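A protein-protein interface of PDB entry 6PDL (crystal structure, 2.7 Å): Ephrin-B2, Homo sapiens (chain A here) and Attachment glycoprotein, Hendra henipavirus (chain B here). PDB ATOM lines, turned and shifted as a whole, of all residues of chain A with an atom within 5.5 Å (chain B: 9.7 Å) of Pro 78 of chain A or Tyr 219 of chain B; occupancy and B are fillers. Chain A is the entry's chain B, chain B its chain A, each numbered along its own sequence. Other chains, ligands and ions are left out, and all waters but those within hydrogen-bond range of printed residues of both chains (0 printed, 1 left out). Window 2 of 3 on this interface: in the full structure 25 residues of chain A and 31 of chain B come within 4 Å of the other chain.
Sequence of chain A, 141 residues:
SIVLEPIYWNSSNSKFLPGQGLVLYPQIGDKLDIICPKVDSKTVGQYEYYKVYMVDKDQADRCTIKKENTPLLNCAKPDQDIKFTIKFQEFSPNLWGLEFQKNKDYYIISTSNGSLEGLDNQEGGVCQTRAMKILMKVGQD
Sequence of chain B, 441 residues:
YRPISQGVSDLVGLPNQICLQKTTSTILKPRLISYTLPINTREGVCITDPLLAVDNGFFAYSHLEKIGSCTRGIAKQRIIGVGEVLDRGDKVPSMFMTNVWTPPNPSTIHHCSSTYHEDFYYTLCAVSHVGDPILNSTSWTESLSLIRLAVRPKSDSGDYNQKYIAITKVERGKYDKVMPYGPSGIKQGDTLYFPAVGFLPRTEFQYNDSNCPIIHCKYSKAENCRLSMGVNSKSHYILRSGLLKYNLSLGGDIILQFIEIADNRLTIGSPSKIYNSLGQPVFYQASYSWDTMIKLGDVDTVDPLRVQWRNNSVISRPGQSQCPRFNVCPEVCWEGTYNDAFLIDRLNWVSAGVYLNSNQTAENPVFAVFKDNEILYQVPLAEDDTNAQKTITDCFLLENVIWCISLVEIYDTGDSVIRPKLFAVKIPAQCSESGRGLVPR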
ATOM      1  N   LYS A  38      18.782  -3.621 -39.785  1.00  0.00           N
ATOM      2  CA  LYS A  38      19.860  -3.627 -38.801  1.00  0.00           C
ATOM      3  C   LYS A  38      20.716  -2.382 -39.013  1.00  0.00           C
ATOM      4  O   LYS A  38      20.703  -1.769 -40.089  1.00  0.00           O
ATOM      5  CB  LYS A  38      20.765  -4.913 -38.979  1.00  0.00           C
ATOM      6  CG  LYS A  38      21.106  -5.548 -37.593  1.00  0.00           C
ATOM      7  CD  LYS A  38      21.825  -6.996 -37.431  1.00  0.00           C
ATOM      8  CE  LYS A  38      23.136  -7.291 -38.277  1.00  0.00           C
ATOM      9  NZ  LYS A  38      23.558  -8.764 -38.157  1.00  0.00           N
ATOM     10  N   VAL A  39      21.448  -1.985 -37.982  1.00  0.00           N
ATOM     11  CA  VAL A  39      22.336  -0.844 -38.202  1.00  0.00           C
ATOM     12  C   VAL A  39      23.772  -1.347 -38.170  1.00  0.00           C
ATOM     13  O   VAL A  39      24.375  -1.575 -39.227  1.00  0.00           O
ATOM     14  CB  VAL A  39      22.140   0.289 -37.193  1.00  0.00           C
ATOM     15  CG1 VAL A  39      22.945   0.031 -35.929  1.00  0.00           C
ATOM     16  CG2 VAL A  39      22.579   1.581 -37.827  1.00  0.00           C
ATOM     17  N   TYR A  47      20.641   4.753 -36.727  1.00  0.00           N
ATOM     18  CA  TYR A  47      19.416   3.967 -36.778  1.00  0.00           C
ATOM     19  C   TYR A  47      18.170   4.845 -36.822  1.00  0.00           C
ATOM     20  O   TYR A  47      18.139   5.939 -36.250  1.00  0.00           O
ATOM     21  CB  TYR A  47      19.381   3.051 -35.554  1.00  0.00           C
ATOM     22  CG  TYR A  47      18.275   2.023 -35.471  1.00  0.00           C
ATOM     23  CD1 TYR A  47      18.165   0.994 -36.407  1.00  0.00           C
ATOM     24  CD2 TYR A  47      17.380   2.043 -34.409  1.00  0.00           C
ATOM     25  CE1 TYR A  47      17.165   0.037 -36.303  1.00  0.00           C
ATOM     26  CE2 TYR A  47      16.384   1.097 -34.296  1.00  0.00           C
ATOM     27  CZ  TYR A  47      16.280   0.095 -35.240  1.00  0.00           C
ATOM     28  OH  TYR A  47      15.279  -0.843 -35.111  1.00  0.00           O
ATOM     29  N   TYR A  49      14.159   4.928 -35.771  1.00  0.00           N
ATOM     30  CA  TYR A  49      13.242   4.328 -34.804  1.00  0.00           C
ATOM     31  C   TYR A  49      11.798   4.530 -35.242  1.00  0.00           C
ATOM     32  O   TYR A  49      11.392   5.658 -35.539  1.00  0.00           O
ATOM     33  CB  TYR A  49      13.424   4.942 -33.416  1.00  0.00           C
ATOM     34  CG  TYR A  49      14.756   4.681 -32.760  1.00  0.00           C
ATOM     35  CD1 TYR A  49      15.862   5.469 -33.054  1.00  0.00           C
ATOM     36  CD2 TYR A  49      14.903   3.661 -31.831  1.00  0.00           C
ATOM     37  CE1 TYR A  49      17.081   5.237 -32.450  1.00  0.00           C
ATOM     38  CE2 TYR A  49      16.117   3.421 -31.222  1.00  0.00           C
ATOM     39  CZ  TYR A  49      17.203   4.214 -31.532  1.00  0.00           C
ATOM     40  OH  TYR A  49      18.414   3.980 -30.924  1.00  0.00           O
ATOM     41  N   ALA A  76      12.942  -0.469 -32.279  1.00  0.00           N
ATOM     42  CA  ALA A  76      13.722   0.241 -31.277  1.00  0.00           C
ATOM     43  C   ALA A  76      14.918  -0.593 -30.832  1.00  0.00           C
ATOM     44  O   ALA A  76      15.340  -0.512 -29.673  1.00  0.00           O
ATOM     45  CB  ALA A  76      12.861   0.618 -30.071  1.00  0.00           C
ATOM     46  N   LYS A  77      15.460  -1.414 -31.735  1.00  0.00           N
ATOM     47  CA  LYS A  77      16.611  -2.269 -31.450  1.00  0.00           C
ATOM     48  C   LYS A  77      17.635  -2.083 -32.559  1.00  0.00           C
ATOM     49  O   LYS A  77      17.614  -2.805 -33.568  1.00  0.00           O
ATOM     50  CB  LYS A  77      16.201  -3.736 -31.343  1.00  0.00           C
ATOM     51  CG  LYS A  77      15.321  -4.081 -30.157  1.00  0.00           C
ATOM     52  CD  LYS A  77      14.882  -5.538 -30.248  1.00  0.00           C
ATOM     53  CE  LYS A  77      14.398  -6.071 -28.909  1.00  0.00           C
ATOM     54  NZ  LYS A  77      13.591  -5.063 -28.171  1.00  0.00           N
ATOM     55  N   PRO A  78      18.564  -1.136 -32.398  1.00  0.00           N
ATOM     56  CA  PRO A  78      19.593  -0.936 -33.431  1.00  0.00           C
ATOM     57  C   PRO A  78      20.441  -2.167 -33.673  1.00  0.00           C
ATOM     58  O   PRO A  78      20.994  -2.326 -34.770  1.00  0.00           O
ATOM     59  CB  PRO A  78      20.438   0.219 -32.873  1.00  0.00           C
ATOM     60  CG  PRO A  78      19.654   0.787 -31.728  1.00  0.00           C
ATOM     61  CD  PRO A  78      18.825  -0.329 -31.197  1.00  0.00           C
ATOM     62  N   ASP A  79      20.559  -3.044 -32.676  1.00  0.00           N
ATOM     63  CA  ASP A  79      21.421  -4.211 -32.804  1.00  0.00           C
ATOM     64  C   ASP A  79      20.818  -5.314 -33.670  1.00  0.00           C
ATOM     65  O   ASP A  79      21.566  -6.058 -34.313  1.00  0.00           O
ATOM     66  CB  ASP A  79      21.744  -4.756 -31.415  1.00  0.00           C
ATOM     67  CG  ASP A  79      23.118  -5.369 -31.342  1.00  0.00           C
ATOM     68  OD1 ASP A  79      23.797  -5.408 -32.388  1.00  0.00           O
ATOM     69  OD2 ASP A  79      23.522  -5.808 -30.247  1.00  0.00           O
ATOM     70  N   GLN A  80      19.494  -5.458 -33.697  1.00  0.00           N
ATOM     71  CA  GLN A  80      18.878  -6.624 -34.313  1.00  0.00           C
ATOM     72  C   GLN A  80      17.994  -6.242 -35.493  1.00  0.00           C
ATOM     73  O   GLN A  80      17.513  -5.112 -35.607  1.00  0.00           O
ATOM     74  CB  GLN A  80      18.043  -7.423 -33.307  1.00  0.00           C
ATOM     75  CG  GLN A  80      18.751  -7.728 -32.002  1.00  0.00           C
ATOM     76  CD  GLN A  80      17.797  -8.215 -30.925  1.00  0.00           C
ATOM     77  OE1 GLN A  80      16.631  -8.513 -31.195  1.00  0.00           O
ATOM     78  NE2 GLN A  80      18.287  -8.292 -29.694  1.00  0.00           N
ATOM     79  N   PRO B 213      13.203 -12.001 -15.515  1.00  0.00           N
ATOM     80  CA  PRO B 213      14.543 -12.454 -15.964  1.00  0.00           C
ATOM     81  C   PRO B 213      15.074 -11.710 -17.187  1.00  0.00           C
ATOM     82  O   PRO B 213      14.972 -12.149 -18.332  1.00  0.00           O
ATOM     83  CB  PRO B 213      14.309 -13.936 -16.268  1.00  0.00           C
ATOM     84  CG  PRO B 213      12.887 -13.996 -16.698  1.00  0.00           C
ATOM     85  CD  PRO B 213      12.150 -12.962 -15.880  1.00  0.00           C
ATOM     86  N   ILE B 214      15.664 -10.534 -16.958  1.00  0.00           N
ATOM     87  CA  ILE B 214      16.123  -9.714 -18.070  1.00  0.00           C
ATOM     88  C   ILE B 214      17.610  -9.875 -18.352  1.00  0.00           C
ATOM     89  O   ILE B 214      18.113  -9.282 -19.318  1.00  0.00           O
ATOM     90  CB  ILE B 214      15.775  -8.231 -17.835  1.00  0.00           C
ATOM     91  CG1 ILE B 214      16.123  -7.807 -16.407  1.00  0.00           C
ATOM     92  CG2 ILE B 214      14.299  -7.999 -18.122  1.00  0.00           C
ATOM     93  CD1 ILE B 214      16.068  -6.308 -16.195  1.00  0.00           C
ATOM     94  N   ILE B 215      18.335 -10.664 -17.554  1.00  0.00           N
ATOM     95  CA  ILE B 215      19.732 -10.938 -17.881  1.00  0.00           C
ATOM     96  C   ILE B 215      19.804 -11.807 -19.139  1.00  0.00           C
ATOM     97  O   ILE B 215      19.004 -12.734 -19.322  1.00  0.00           O
ATOM     98  CB  ILE B 215      20.491 -11.526 -16.671  1.00  0.00           C
ATOM     99  CG1 ILE B 215      21.997 -11.587 -16.973  1.00  0.00           C
ATOM    100  CG2 ILE B 215      19.913 -12.865 -16.213  1.00  0.00           C
ATOM    101  CD1 ILE B 215      22.526 -10.334 -17.651  1.00  0.00           C
ATOM    102  N   HIS B 216      20.782 -11.506 -20.007  1.00  0.00           N
ATOM    103  CA  HIS B 216      20.973 -11.982 -21.386  1.00  0.00           C
ATOM    104  C   HIS B 216      19.959 -11.389 -22.350  1.00  0.00           C
ATOM    105  O   HIS B 216      19.832 -11.873 -23.480  1.00  0.00           O
ATOM    106  CB  HIS B 216      20.892 -13.510 -21.596  1.00  0.00           C
ATOM    107  CG  HIS B 216      21.725 -14.366 -20.682  1.00  0.00           C
ATOM    108  ND1 HIS B 216      21.272 -14.844 -19.470  1.00  0.00           N
ATOM    109  CD2 HIS B 216      22.972 -14.870 -20.839  1.00  0.00           C
ATOM    110  CE1 HIS B 216      22.200 -15.615 -18.927  1.00  0.00           C
ATOM    111  NE2 HIS B 216      23.248 -15.635 -19.730  1.00  0.00           N
ATOM    112  N   CYS B 217      19.228 -10.359 -21.943  1.00  0.00           N
ATOM    113  CA  CYS B 217      18.285  -9.681 -22.831  1.00  0.00           C
ATOM    114  C   CYS B 217      18.484  -8.183 -22.630  1.00  0.00           C
ATOM    115  O   CYS B 217      17.801  -7.562 -21.812  1.00  0.00           O
ATOM    116  CB  CYS B 217      16.873 -10.129 -22.521  1.00  0.00           C
ATOM    117  SG  CYS B 217      16.688 -11.913 -22.441  1.00  0.00           S
ATOM    118  N   LYS B 218      19.434  -7.608 -23.371  1.00  0.00           N
ATOM    119  CA  LYS B 218      19.865  -6.240 -23.106  1.00  0.00           C
ATOM    120  C   LYS B 218      18.777  -5.218 -23.399  1.00  0.00           C
ATOM    121  O   LYS B 218      18.809  -4.118 -22.837  1.00  0.00           O
ATOM    122  CB  LYS B 218      21.095  -5.910 -23.947  1.00  0.00           C
ATOM    123  CG  LYS B 218      20.825  -6.042 -25.430  1.00  0.00           C
ATOM    124  CD  LYS B 218      21.879  -5.355 -26.255  1.00  0.00           C
ATOM    125  CE  LYS B 218      22.374  -6.273 -27.349  1.00  0.00           C
ATOM    126  NZ  LYS B 218      23.562  -5.697 -28.030  1.00  0.00           N
ATOM    127  N   TYR B 219      17.811  -5.554 -24.252  1.00  0.00           N
ATOM    128  CA  TYR B 219      16.744  -4.621 -24.569  1.00  0.00           C
ATOM    129  C   TYR B 219      15.527  -4.763 -23.675  1.00  0.00           C
ATOM    130  O   TYR B 219      14.637  -3.909 -23.733  1.00  0.00           O
ATOM    131  CB  TYR B 219      16.316  -4.796 -26.024  1.00  0.00           C
ATOM    132  CG  TYR B 219      17.322  -4.243 -26.993  1.00  0.00           C
ATOM    133  CD1 TYR B 219      18.000  -5.077 -27.865  1.00  0.00           C
ATOM    134  CD2 TYR B 219      17.607  -2.885 -27.024  1.00  0.00           C
ATOM    135  CE1 TYR B 219      18.927  -4.580 -28.749  1.00  0.00           C
ATOM    136  CE2 TYR B 219      18.532  -2.377 -27.904  1.00  0.00           C
ATOM    137  CZ  TYR B 219      19.191  -3.231 -28.766  1.00  0.00           C
ATOM    138  OH  TYR B 219      20.121  -2.743 -29.654  1.00  0.00           O
ATOM    139  N   SER B 220      15.469  -5.793 -22.843  1.00  0.00           N
ATOM    140  CA  SER B 220      14.312  -5.982 -21.988  1.00  0.00           C
ATOM    141  C   SER B 220      14.494  -5.205 -20.693  1.00  0.00           C
ATOM    142  O   SER B 220      15.615  -5.003 -20.220  1.00  0.00           O
ATOM    143  CB  SER B 220      14.097  -7.469 -21.707  1.00  0.00           C
ATOM    144  OG  SER B 220      13.981  -8.192 -22.924  1.00  0.00           O
ATOM    145  N   LYS B 221      13.376  -4.791 -20.114  1.00  0.00           N
ATOM    146  CA  LYS B 221      13.353  -4.028 -18.878  1.00  0.00           C
ATOM    147  C   LYS B 221      12.615  -4.816 -17.806  1.00  0.00           C
ATOM    148  O   LYS B 221      11.820  -5.708 -18.104  1.00  0.00           O
ATOM    149  CB  LYS B 221      12.704  -2.655 -19.091  1.00  0.00           C
ATOM    150  CG  LYS B 221      13.468  -1.777 -20.075  1.00  0.00           C
ATOM    151  CD  LYS B 221      12.559  -0.798 -20.798  1.00  0.00           C
ATOM    152  CE  LYS B 221      13.370   0.296 -21.482  1.00  0.00           C
ATOM    153  NZ  LYS B 221      12.536   1.120 -22.402  1.00  0.00           N
ATOM    154  N   ALA B 222      12.898  -4.483 -16.544  1.00  0.00           N
ATOM    155  CA  ALA B 222      12.355  -5.242 -15.421  1.00  0.00           C
ATOM    156  C   ALA B 222      10.834  -5.206 -15.358  1.00  0.00           C
ATOM    157  O   ALA B 222      10.227  -6.112 -14.776  1.00  0.00           O
ATOM    158  CB  ALA B 222      12.916  -4.706 -14.105  1.00  0.00           C
ATOM    159  N   GLU B 223      10.207  -4.185 -15.935  1.00  0.00           N
ATOM    160  CA  GLU B 223       8.758  -4.048 -15.891  1.00  0.00           C
ATOM    161  C   GLU B 223       8.035  -4.920 -16.907  1.00  0.00           C
ATOM    162  O   GLU B 223       6.802  -4.995 -16.861  1.00  0.00           O
ATOM    163  CB  GLU B 223       8.378  -2.591 -16.139  1.00  0.00           C
ATOM    164  CG  GLU B 223       8.811  -2.133 -17.523  1.00  0.00           C
ATOM    165  CD  GLU B 223       8.676  -0.646 -17.731  1.00  0.00           C
ATOM    166  OE1 GLU B 223       8.255   0.054 -16.783  1.00  0.00           O
ATOM    167  OE2 GLU B 223       8.999  -0.179 -18.845  1.00  0.00           O
ATOM    168  N   ASN B 224       8.761  -5.563 -17.824  1.00  0.00           N
ATOM    169  CA  ASN B 224       8.116  -6.195 -18.968  1.00  0.00           C
ATOM    170  C   ASN B 224       7.227  -7.364 -18.549  1.00  0.00           C
ATOM    171  O   ASN B 224       6.148  -7.559 -19.117  1.00  0.00           O
ATOM    172  CB  ASN B 224       9.175  -6.648 -19.973  1.00  0.00           C
ATOM    173  CG  ASN B 224       9.696  -5.502 -20.824  1.00  0.00           C
ATOM    174  OD1 ASN B 224       9.201  -4.378 -20.729  1.00  0.00           O
ATOM    175  ND2 ASN B 224      10.701  -5.778 -21.657  1.00  0.00           N
ATOM    176  N   GLN B 322       6.828  -8.812 -32.045  1.00  0.00           N
ATOM    177  CA  GLN B 322       7.529  -8.599 -30.777  1.00  0.00           C
ATOM    178  C   GLN B 322       7.987  -9.901 -30.129  1.00  0.00           C
ATOM    179  O   GLN B 322       9.095  -9.969 -29.576  1.00  0.00           O
ATOM    180  CB  GLN B 322       6.631  -7.817 -29.822  1.00  0.00           C
ATOM    181  CG  GLN B 322       7.355  -7.300 -28.602  1.00  0.00           C
ATOM    182  CD  GLN B 322       7.950  -5.931 -28.829  1.00  0.00           C
ATOM    183  OE1 GLN B 322       8.983  -5.795 -29.487  1.00  0.00           O
ATOM    184  NE2 GLN B 322       7.297  -4.902 -28.293  1.00  0.00           N
ATOM    185  N   ASN B 327      11.103 -16.887 -29.198  1.00  0.00           N
ATOM    186  CA  ASN B 327      11.422 -15.771 -28.322  1.00  0.00           C
ATOM    187  C   ASN B 327      11.477 -16.259 -26.883  1.00  0.00           C
ATOM    188  O   ASN B 327      10.629 -17.038 -26.443  1.00  0.00           O
ATOM    189  CB  ASN B 327      10.375 -14.663 -28.466  1.00  0.00           C
ATOM    190  CG  ASN B 327      10.753 -13.388 -27.728  1.00  0.00           C
ATOM    191  OD1 ASN B 327      11.540 -12.577 -28.223  1.00  0.00           O
ATOM    192  ND2 ASN B 327      10.173 -13.194 -26.549  1.00  0.00           N
ATOM    193  N   CYS B 329      13.012 -13.748 -24.427  1.00  0.00           N
ATOM    194  CA  CYS B 329      13.333 -12.561 -23.643  1.00  0.00           C
ATOM    195  C   CYS B 329      12.078 -11.736 -23.367  1.00  0.00           C
ATOM    196  O   CYS B 329      11.263 -11.515 -24.274  1.00  0.00           O
ATOM    197  CB  CYS B 329      14.356 -11.703 -24.383  1.00  0.00           C
ATOM    198  SG  CYS B 329      16.028 -12.381 -24.338  1.00  0.00           S
ATOM    199  N   PRO B 330      11.918 -11.266 -22.130  1.00  0.00           N
ATOM    200  CA  PRO B 330      10.672 -10.579 -21.742  1.00  0.00           C
ATOM    201  C   PRO B 330      10.386  -9.338 -22.579  1.00  0.00           C
ATOM    202  O   PRO B 330      11.146  -8.368 -22.569  1.00  0.00           O
ATOM    203  CB  PRO B 330      10.916 -10.223 -20.276  1.00  0.00           C
ATOM    204  CG  PRO B 330      11.893 -11.257 -19.792  1.00  0.00           C
ATOM    205  CD  PRO B 330      12.768 -11.593 -20.971  1.00  0.00           C
ATOM    206  N   GLU B 331       9.266  -9.375 -23.299  1.00  0.00           N
ATOM    207  CA  GLU B 331       8.743  -8.236 -24.039  1.00  0.00           C
ATOM    208  C   GLU B 331       7.298  -8.027 -23.620  1.00  0.00           C
ATOM    209  O   GLU B 331       6.695  -8.883 -22.969  1.00  0.00           O
ATOM    210  CB  GLU B 331       8.832  -8.446 -25.558  1.00  0.00           C
ATOM    211  CG  GLU B 331      10.129  -9.083 -26.031  1.00  0.00           C
ATOM    212  CD  GLU B 331      11.240  -8.065 -26.220  1.00  0.00           C
ATOM    213  OE1 GLU B 331      11.001  -6.873 -25.937  1.00  0.00           O
ATOM    214  OE2 GLU B 331      12.347  -8.452 -26.656  1.00  0.00           O
ATOM    215  N   VAL B 332       6.730  -6.882 -23.985  1.00  0.00           N
ATOM    216  CA  VAL B 332       5.321  -6.604 -23.732  1.00  0.00           C
ATOM    217  C   VAL B 332       4.559  -6.935 -25.009  1.00  0.00           C
ATOM    218  O   VAL B 332       4.548  -6.160 -25.970  1.00  0.00           O
ATOM    219  CB  VAL B 332       5.102  -5.162 -23.274  1.00  0.00           C
ATOM    220  CG1 VAL B 332       3.753  -5.012 -22.578  1.00  0.00           C
ATOM    221  CG2 VAL B 332       6.219  -4.756 -22.339  1.00  0.00           C
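Among the printed residues, merely in contact across the chains: Pro 78 of chain A with Tyr 219 of chain B (3.1 Å), Lys 77 of chain A with Tyr 219 of chain B (3.5 Å) and Gln 80 of chain A with Tyr 219 of chain B (3.7 Å).
The backbone carbonyl oxygen (O) of Pro 78 of chain A lies within hydrogen-bond range of the backbone NH (N) of Val 39 of chain A. The side-chain hydroxyl (OH) of Tyr 47 of chain A sits at hydrogen-bond distance from the backbone carbonyl oxygen (O) of Lys 77 of chain A. SG of Cys 217 of chain B is disulfide-bonded to SG of Cys 329 of chain B, 2.1 Å away.
The side-chain hydroxyl (OH) of Tyr 219 of chain B lies within hydrogen-bond range of the backbone NH (N) of Asp 79 of chain A (3.1 Å). NZ of Lys 77 of chain A lies within salt-bridge range of OE1 of Glu 331 of chain B. The side-chain amino group of Lys 218 of chain B lies close to the side-chain carboxylate of Asp 79 of chain A, at 2.2 Å.
Of chain B, only Tyr 219 comes within 4 Å of Pro 78 of chain A. Of chain A, only Lys 77 (3.5 Å), Pro 78 (3.1 Å), Asp 79 (3.1 Å) and Gln 80 (3.7 Å) come within 4 Å of Tyr 219 of chain B. No residue of chain B comes within 4 Å of Val 39 of chain A. Lys 77 of chain A touches just these residues of chain B: Tyr 219 and Glu 331. Of chain B, only Lys 218 and Tyr 219 come within 4 Å of Asp 79 of chain A. Of the printed residues of chain B, Gln 80 of chain A touches Tyr 219 (3.7 Å). Of the printed residues of chain A, Lys 218 of chain B touches Asp 79 (2.2 Å). Printed residues of chain A within 4 Å of Glu 331 of chain B: Lys 77 (3.9 Å). The nearest printed residue of chain A that does not touch Lys 218 of chain B is Gln 80 of chain A (5.1 Å).
Of the 9 printed residues of chain A, 4 touch a printed residue of chain B. Along chain A the printed residues that touch a printed residue of chain B span positions 77 to 80. Printed residues of chain B that touch a printed residue of chain A: Lys 218, Tyr 219 and Glu 331. Hydrophobic or aromatic side chains of chain B within 4 Å of the printed part of chain A: Tyr 219. Among the printed residues, 6 pairs touch across the chains.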
